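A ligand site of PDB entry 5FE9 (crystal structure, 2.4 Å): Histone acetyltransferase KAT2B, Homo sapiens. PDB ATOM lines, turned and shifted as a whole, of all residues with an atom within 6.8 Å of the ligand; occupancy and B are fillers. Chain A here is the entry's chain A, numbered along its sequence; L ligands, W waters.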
ATOM      1  N   TRP A  34     -10.093  -3.725 -11.652  1.00  0.00           N
ATOM      2  CA  TRP A  34     -11.497  -3.461 -12.072  1.00  0.00           C
ATOM      3  C   TRP A  34     -12.174  -2.275 -11.364  1.00  0.00           C
ATOM      4  O   TRP A  34     -12.919  -1.571 -11.985  1.00  0.00           O
ATOM      5  CB  TRP A  34     -12.354  -4.741 -11.993  1.00  0.00           C
ATOM      6  CG  TRP A  34     -12.512  -5.281 -10.586  1.00  0.00           C
ATOM      7  CD1 TRP A  34     -11.738  -6.227  -9.978  1.00  0.00           C
ATOM      8  CD2 TRP A  34     -13.462  -4.861  -9.618  1.00  0.00           C
ATOM      9  NE1 TRP A  34     -12.157  -6.428  -8.699  1.00  0.00           N
ATOM     10  CE2 TRP A  34     -13.221  -5.592  -8.444  1.00  0.00           C
ATOM     11  CE3 TRP A  34     -14.493  -3.914  -9.621  1.00  0.00           C
ATOM     12  CZ2 TRP A  34     -13.967  -5.419  -7.290  1.00  0.00           C
ATOM     13  CZ3 TRP A  34     -15.233  -3.742  -8.481  1.00  0.00           C
ATOM     14  CH2 TRP A  34     -14.986  -4.502  -7.334  1.00  0.00           C
ATOM     15  N   PRO A  35     -11.849  -2.002 -10.088  1.00  0.00           N
ATOM     16  CA  PRO A  35     -12.453  -0.777  -9.519  1.00  0.00           C
ATOM     17  C   PRO A  35     -11.949   0.542 -10.083  1.00  0.00           C
ATOM     18  O   PRO A  35     -12.575   1.584  -9.866  1.00  0.00           O
ATOM     19  CB  PRO A  35     -12.037  -0.840  -8.044  1.00  0.00           C
ATOM     20  CG  PRO A  35     -11.576  -2.225  -7.808  1.00  0.00           C
ATOM     21  CD  PRO A  35     -10.971  -2.653  -9.094  1.00  0.00           C
ATOM     22  N   PHE A  36     -10.801   0.518 -10.765  1.00  0.00           N
ATOM     23  CA  PHE A  36     -10.108   1.741 -11.122  1.00  0.00           C
ATOM     24  C   PHE A  36     -10.092   2.033 -12.616  1.00  0.00           C
ATOM     25  O   PHE A  36      -9.311   2.888 -13.043  1.00  0.00           O
ATOM     26  CB  PHE A  36      -8.661   1.643 -10.594  1.00  0.00           C
ATOM     27  CG  PHE A  36      -8.580   1.204  -9.156  1.00  0.00           C
ATOM     28  CD1 PHE A  36      -9.076   2.019  -8.162  1.00  0.00           C
ATOM     29  CD2 PHE A  36      -8.060  -0.037  -8.821  1.00  0.00           C
ATOM     30  CE1 PHE A  36      -9.056   1.616  -6.850  1.00  0.00           C
ATOM     31  CE2 PHE A  36      -8.032  -0.446  -7.506  1.00  0.00           C
ATOM     32  CZ  PHE A  36      -8.522   0.375  -6.517  1.00  0.00           C
ATOM     33  N   MET A  37     -10.915   1.336 -13.405  1.00  0.00           N
ATOM     34  CA  MET A  37     -10.860   1.407 -14.877  1.00  0.00           C
ATOM     35  C   MET A  37     -11.529   2.647 -15.446  1.00  0.00           C
ATOM     36  O   MET A  37     -11.129   3.127 -16.485  1.00  0.00           O
ATOM     37  CB  MET A  37     -11.498   0.170 -15.513  1.00  0.00           C
ATOM     38  CG  MET A  37     -10.783  -1.139 -15.201  1.00  0.00           C
ATOM     39  SD  MET A  37      -9.150  -1.200 -15.973  1.00  0.00           S
ATOM     40  CE  MET A  37      -9.649  -1.415 -17.656  1.00  0.00           C
ATOM     41  N   GLU A  38     -12.512   3.207 -14.742  1.00  0.00           N
ATOM     42  CA  GLU A  38     -13.115   4.477 -15.160  1.00  0.00           C
ATOM     43  C   GLU A  38     -13.415   5.395 -13.952  1.00  0.00           C
ATOM     44  O   GLU A  38     -13.350   4.950 -12.828  1.00  0.00           O
ATOM     45  CB  GLU A  38     -14.342   4.236 -16.071  1.00  0.00           C
ATOM     46  CG  GLU A  38     -15.600   3.679 -15.456  1.00  0.00           C
ATOM     47  CD  GLU A  38     -16.735   3.682 -16.479  1.00  0.00           C
ATOM     48  OE1 GLU A  38     -17.422   2.653 -16.624  1.00  0.00           O
ATOM     49  OE2 GLU A  38     -16.918   4.710 -17.164  1.00  0.00           O
ATOM     50  N   PRO A  39     -13.665   6.702 -14.202  1.00  0.00           N
ATOM     51  CA  PRO A  39     -13.998   7.667 -13.133  1.00  0.00           C
ATOM     52  C   PRO A  39     -15.109   7.197 -12.186  1.00  0.00           C
ATOM     53  O   PRO A  39     -16.092   6.598 -12.646  1.00  0.00           O
ATOM     54  CB  PRO A  39     -14.469   8.900 -13.901  1.00  0.00           C
ATOM     55  CG  PRO A  39     -13.718   8.849 -15.178  1.00  0.00           C
ATOM     56  CD  PRO A  39     -13.549   7.400 -15.515  1.00  0.00           C
ATOM     57  N   VAL A  40     -14.938   7.459 -10.893  1.00  0.00           N
ATOM     58  CA  VAL A  40     -15.993   7.194  -9.895  1.00  0.00           C
ATOM     59  C   VAL A  40     -17.244   7.976 -10.290  1.00  0.00           C
ATOM     60  O   VAL A  40     -17.151   9.160 -10.605  1.00  0.00           O
ATOM     61  CB  VAL A  40     -15.568   7.571  -8.439  1.00  0.00           C
ATOM     62  CG1 VAL A  40     -16.730   7.384  -7.459  1.00  0.00           C
ATOM     63  CG2 VAL A  40     -14.390   6.712  -7.990  1.00  0.00           C
ATOM     64  N   LYS A  41     -18.394   7.315 -10.265  1.00  0.00           N
ATOM     65  CA  LYS A  41     -19.661   7.978 -10.565  1.00  0.00           C
ATOM     66  C   LYS A  41     -20.255   8.547  -9.277  1.00  0.00           C
ATOM     67  O   LYS A  41     -20.319   7.849  -8.250  1.00  0.00           O
ATOM     68  CB  LYS A  41     -20.649   7.021 -11.212  1.00  0.00           C
ATOM     69  CG  LYS A  41     -20.083   6.231 -12.384  1.00  0.00           C
ATOM     70  CD  LYS A  41     -21.105   5.230 -12.929  1.00  0.00           C
ATOM     71  CE  LYS A  41     -20.631   4.694 -14.301  1.00  0.00           C
ATOM     72  NZ  LYS A  41     -19.757   3.518 -14.130  1.00  0.00           N
ATOM     73  N   ARG A  42     -20.687   9.821  -9.336  1.00  0.00           N
ATOM     74  CA  ARG A  42     -21.351  10.497  -8.219  1.00  0.00           C
ATOM     75  C   ARG A  42     -22.537   9.710  -7.668  1.00  0.00           C
ATOM     76  O   ARG A  42     -22.742   9.627  -6.445  1.00  0.00           O
ATOM     77  CB  ARG A  42     -21.874  11.858  -8.688  1.00  0.00           C
ATOM     78  CG  ARG A  42     -20.780  12.863  -9.037  1.00  0.00           C
ATOM     79  CD  ARG A  42     -21.159  14.241  -8.528  1.00  0.00           C
ATOM     80  NE  ARG A  42     -20.088  15.208  -8.793  1.00  0.00           N
ATOM     81  CZ  ARG A  42     -19.776  16.254  -8.009  1.00  0.00           C
ATOM     82  NH1 ARG A  42     -18.774  17.054  -8.355  1.00  0.00           N
ATOM     83  NH2 ARG A  42     -20.451  16.500  -6.880  1.00  0.00           N
ATOM     84  N   GLU A  44     -22.938   6.493  -7.730  1.00  0.00           N
ATOM     85  CA  GLU A  44     -22.456   5.291  -7.027  1.00  0.00           C
ATOM     86  C   GLU A  44     -21.645   5.579  -5.742  1.00  0.00           C
ATOM     87  O   GLU A  44     -21.336   4.645  -5.011  1.00  0.00           O
ATOM     88  CB  GLU A  44     -21.660   4.408  -7.998  1.00  0.00           C
ATOM     89  CG  GLU A  44     -22.406   4.089  -9.300  1.00  0.00           C
ATOM     90  CD  GLU A  44     -22.055   2.738  -9.907  1.00  0.00           C
ATOM     91  OE1 GLU A  44     -22.966   2.065 -10.464  1.00  0.00           O
ATOM     92  OE2 GLU A  44     -20.878   2.345  -9.844  1.00  0.00           O
ATOM     93  N   ALA A  45     -21.281   6.845  -5.471  1.00  0.00           N
ATOM     94  CA  ALA A  45     -20.499   7.157  -4.230  1.00  0.00           C
ATOM     95  C   ALA A  45     -20.777   8.488  -3.561  1.00  0.00           C
ATOM     96  O   ALA A  45     -20.140   9.493  -3.906  1.00  0.00           O
ATOM     97  CB  ALA A  45     -19.014   7.058  -4.526  1.00  0.00           C
ATOM     98  N   PRO A  46     -21.646   8.489  -2.518  1.00  0.00           N
ATOM     99  CA  PRO A  46     -22.074   9.783  -1.990  1.00  0.00           C
ATOM    100  C   PRO A  46     -20.949  10.555  -1.319  1.00  0.00           C
ATOM    101  O   PRO A  46     -20.027   9.969  -0.700  1.00  0.00           O
ATOM    102  CB  PRO A  46     -23.184   9.415  -0.984  1.00  0.00           C
ATOM    103  CG  PRO A  46     -23.584   8.021  -1.329  1.00  0.00           C
ATOM    104  CD  PRO A  46     -22.319   7.379  -1.816  1.00  0.00           C
ATOM    105  N   TYR A  48     -18.361  11.606  -2.401  1.00  0.00           N
ATOM    106  CA  TYR A  48     -17.009  11.234  -2.842  1.00  0.00           C
ATOM    107  C   TYR A  48     -16.235  12.464  -3.287  1.00  0.00           C
ATOM    108  O   TYR A  48     -15.075  12.643  -2.912  1.00  0.00           O
ATOM    109  CB  TYR A  48     -17.029  10.203  -3.977  1.00  0.00           C
ATOM    110  CG  TYR A  48     -15.650   9.722  -4.435  1.00  0.00           C
ATOM    111  CD1 TYR A  48     -14.929  10.415  -5.409  1.00  0.00           C
ATOM    112  CD2 TYR A  48     -15.083   8.559  -3.896  1.00  0.00           C
ATOM    113  CE1 TYR A  48     -13.676   9.968  -5.821  1.00  0.00           C
ATOM    114  CE2 TYR A  48     -13.830   8.105  -4.316  1.00  0.00           C
ATOM    115  CZ  TYR A  48     -13.129   8.798  -5.275  1.00  0.00           C
ATOM    116  OH  TYR A  48     -11.882   8.344  -5.682  1.00  0.00           O
ATOM    117  N   ASP A  57      -8.188   7.855 -12.427  1.00  0.00           N
ATOM    118  CA  ASP A  57      -8.535   6.496 -12.842  1.00  0.00           C
ATOM    119  C   ASP A  57      -7.725   6.115 -14.064  1.00  0.00           C
ATOM    120  O   ASP A  57      -7.165   6.969 -14.733  1.00  0.00           O
ATOM    121  CB  ASP A  57     -10.004   6.417 -13.175  1.00  0.00           C
ATOM    122  CG  ASP A  57     -10.348   7.236 -14.389  1.00  0.00           C
ATOM    123  OD1 ASP A  57     -10.533   8.452 -14.263  1.00  0.00           O
ATOM    124  OD2 ASP A  57     -10.365   6.643 -15.478  1.00  0.00           O
ATOM    125  N   VAL A  83      -4.528   7.232  -7.649  1.00  0.00           N
ATOM    126  CA  VAL A  83      -5.603   6.267  -7.770  1.00  0.00           C
ATOM    127  C   VAL A  83      -5.714   5.464  -6.476  1.00  0.00           C
ATOM    128  O   VAL A  83      -6.820   5.222  -5.956  1.00  0.00           O
ATOM    129  CB  VAL A  83      -5.369   5.306  -8.952  1.00  0.00           C
ATOM    130  CG1 VAL A  83      -6.394   4.166  -8.948  1.00  0.00           C
ATOM    131  CG2 VAL A  83      -5.394   6.044 -10.287  1.00  0.00           C
ATOM    132  N   ASN A  86      -6.452   7.813  -3.129  1.00  0.00           N
ATOM    133  CA  ASN A  86      -7.864   8.198  -3.132  1.00  0.00           C
ATOM    134  C   ASN A  86      -8.741   7.045  -2.601  1.00  0.00           C
ATOM    135  O   ASN A  86      -9.556   7.206  -1.678  1.00  0.00           O
ATOM    136  CB  ASN A  86      -8.341   8.556  -4.532  1.00  0.00           C
ATOM    137  CG  ASN A  86      -7.803   9.886  -5.043  1.00  0.00           C
ATOM    138  OD1 ASN A  86      -7.265  10.704  -4.295  1.00  0.00           O
ATOM    139  ND2 ASN A  86      -7.975  10.116  -6.347  1.00  0.00           N
ATOM    140  N   CYS A  87      -8.535   5.882  -3.182  1.00  0.00           N
ATOM    141  CA  CYS A  87      -9.276   4.710  -2.785  1.00  0.00           C
ATOM    142  C   CYS A  87      -9.105   4.391  -1.295  1.00  0.00           C
ATOM    143  O   CYS A  87     -10.087   4.080  -0.611  1.00  0.00           O
ATOM    144  CB  CYS A  87      -8.823   3.528  -3.637  1.00  0.00           C
ATOM    145  SG  CYS A  87      -9.689   1.998  -3.240  1.00  0.00           S
ATOM    146  N   LYS A  88      -7.875   4.483  -0.803  1.00  0.00           N
ATOM    147  CA  LYS A  88      -7.615   4.124   0.573  1.00  0.00           C
ATOM    148  C   LYS A  88      -8.156   5.132   1.543  1.00  0.00           C
ATOM    149  O   LYS A  88      -8.552   4.732   2.659  1.00  0.00           O
ATOM    150  CB  LYS A  88      -6.137   3.872   0.786  1.00  0.00           C
ATOM    151  CG  LYS A  88      -5.704   2.627   0.089  1.00  0.00           C
ATOM    152  CD  LYS A  88      -4.294   2.142   0.493  1.00  0.00           C
ATOM    153  CE  LYS A  88      -3.314   2.379  -0.606  1.00  0.00           C
ATOM    154  NZ  LYS A  88      -1.949   1.982  -0.231  1.00  0.00           N
ATOM    155  N   TYR A  90     -10.917   7.042   1.004  1.00  0.00           N
ATOM    156  CA  TYR A  90     -12.364   7.009   0.941  1.00  0.00           C
ATOM    157  C   TYR A  90     -12.962   5.736   1.525  1.00  0.00           C
ATOM    158  O   TYR A  90     -13.946   5.791   2.223  1.00  0.00           O
ATOM    159  CB  TYR A  90     -12.830   7.170  -0.482  1.00  0.00           C
ATOM    160  CG  TYR A  90     -14.323   7.346  -0.569  1.00  0.00           C
ATOM    161  CD1 TYR A  90     -14.915   8.540  -0.155  1.00  0.00           C
ATOM    162  CD2 TYR A  90     -15.161   6.301  -1.025  1.00  0.00           C
ATOM    163  CE1 TYR A  90     -16.301   8.705  -0.188  1.00  0.00           C
ATOM    164  CE2 TYR A  90     -16.539   6.460  -1.054  1.00  0.00           C
ATOM    165  CZ  TYR A  90     -17.103   7.656  -0.644  1.00  0.00           C
ATOM    166  OH  TYR A  90     -18.459   7.832  -0.726  1.00  0.00           O
ATOM    167  N   ASN A  91     -12.364   4.584   1.244  1.00  0.00           N
ATOM    168  CA  ASN A  91     -12.964   3.306   1.627  1.00  0.00           C
ATOM    169  C   ASN A  91     -12.456   2.715   2.969  1.00  0.00           C
ATOM    170  O   ASN A  91     -11.298   2.911   3.343  1.00  0.00           O
ATOM    171  CB  ASN A  91     -12.703   2.305   0.528  1.00  0.00           C
ATOM    172  CG  ASN A  91     -13.398   2.692  -0.767  1.00  0.00           C
ATOM    173  OD1 ASN A  91     -14.594   2.494  -0.918  1.00  0.00           O
ATOM    174  ND2 ASN A  91     -12.649   3.239  -1.702  1.00  0.00           N
ATOM    175  N   TYR A  97     -12.482  -2.806  -2.201  1.00  0.00           N
ATOM    176  CA  TYR A  97     -11.810  -1.721  -2.934  1.00  0.00           C
ATOM    177  C   TYR A  97     -10.436  -1.422  -2.361  1.00  0.00           C
ATOM    178  O   TYR A  97      -9.479  -1.279  -3.114  1.00  0.00           O
ATOM    179  CB  TYR A  97     -12.648  -0.430  -2.968  1.00  0.00           C
ATOM    180  CG  TYR A  97     -13.955  -0.571  -3.724  1.00  0.00           C
ATOM    181  CD1 TYR A  97     -13.999  -1.101  -5.003  1.00  0.00           C
ATOM    182  CD2 TYR A  97     -15.153  -0.145  -3.156  1.00  0.00           C
ATOM    183  CE1 TYR A  97     -15.187  -1.206  -5.692  1.00  0.00           C
ATOM    184  CE2 TYR A  97     -16.347  -0.256  -3.840  1.00  0.00           C
ATOM    185  CZ  TYR A  97     -16.354  -0.783  -5.111  1.00  0.00           C
ATOM    186  OH  TYR A  97     -17.532  -0.897  -5.781  1.00  0.00           O
HETATM  187  C1  LIG L   1     -17.565   3.861  -3.718  1.00  0.00           C
HETATM  188  C2  LIG L   1     -16.484   3.647  -4.603  1.00  0.00           C
HETATM  189  C3  LIG L   1     -15.217   3.916  -4.114  1.00  0.00           C
HETATM  190  C4  LIG L   1     -14.091   3.722  -4.902  1.00  0.00           C
HETATM  191  O1  LIG L   1     -12.987   3.972  -4.414  1.00  0.00           O
HETATM  192  N1  LIG L   1     -14.195   3.270  -6.163  1.00  0.00           N
HETATM  193  C5  LIG L   1     -12.920   3.094  -6.949  1.00  0.00           C
HETATM  194  C6  LIG L   1     -15.430   2.984  -6.691  1.00  0.00           C
HETATM  195  C7  LIG L   1     -15.582   2.514  -8.011  1.00  0.00           C
HETATM  196  C8  LIG L   1     -16.607   3.167  -5.917  1.00  0.00           C
HETATM  197  C9  LIG L   1     -17.867   2.872  -6.488  1.00  0.00           C
HETATM  198  C10 LIG L   1     -17.975   2.406  -7.788  1.00  0.00           C
HETATM  199  C11 LIG L   1     -16.833   2.232  -8.555  1.00  0.00           C
HETATM  200  N2  LIG L   1     -16.928   1.781  -9.804  1.00  0.00           N
HETATM  201  S1  LIG L   1     -17.066   2.902 -11.081  1.00  0.00           S
HETATM  202  O2  LIG L   1     -18.126   3.953 -10.729  1.00  0.00           O
HETATM  203  O3  LIG L   1     -15.734   3.599 -11.351  1.00  0.00           O
HETATM  204  C12 LIG L   1     -17.508   1.961 -12.532  1.00  0.00           C
HETATM  205  O   HOH W   1     -14.270   0.875 -12.774  1.00  0.00           O
HETATM  206  O   HOH W   2     -15.852  -0.324 -10.583  1.00  0.00           O
HETATM  207  O   HOH W   3     -11.176   6.024  -5.198  1.00  0.00           O
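The side-chain amide nitrogen of Asn 91 sits at hydrogen-bond distance from an oxygen (O1) of the ligand, 2.8 Å away. An oxygen (O2) of the ligand sits at hydrogen-bond distance from the backbone NH (N) of Lys 41, 3.4 Å away.
The side-chain amide nitrogen of Asn 91 is in hydrogen-bond range of the backbone carbonyl oxygen of Cys 87, at 2.9 Å. NZ of Lys 41 lies within salt-bridge range of OE1 of Glu 38 (3.5 Å). O of Tyr 97 lies within hydrogen-bond range of SG of Cys 87. The side-chain hydroxyl of Tyr 90 sits at hydrogen-bond distance from the backbone carbonyl oxygen of Pro 46 (2.7 Å).
The backbone carbonyl oxygen of Glu 38 lies close to an oxygen (O3) of the ligand (3.1 Å). The backbone carbonyl oxygen (O) of Pro 39 sits close to an oxygen (O3) of the ligand (3.3 Å). The side-chain carboxylate of Glu 44 sits close to an oxygen (O2) of the ligand, at 3.3 Å. Merely in contact with the ligand: Pro 35 (3.3 Å), Val 40 (3.9 Å), Ala 45 (3.6 Å), Tyr 90 (3.9 Å) and Tyr 97 (3.8 Å). Hydrophobic or aromatic side chains that line the ligand: Val 40, Ala 45, Tyr 90 and Tyr 97. Of the 21 residues printed, 10 come within 4 Å of the ligand. The nearest printed residue that does not touch the ligand is Cys 87 (4.02 Å).
Water W2 bridges a nitrogen (N2) of the ligand (2.5 Å) and the backbone carbonyl oxygen of Trp 34 (3.5 Å). Water W3 lies within hydrogen-bond range of OH of Tyr 48 (2.5 Å), O1 of the ligand (2.8 Å) and N of Cys 87 (3.3 Å).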
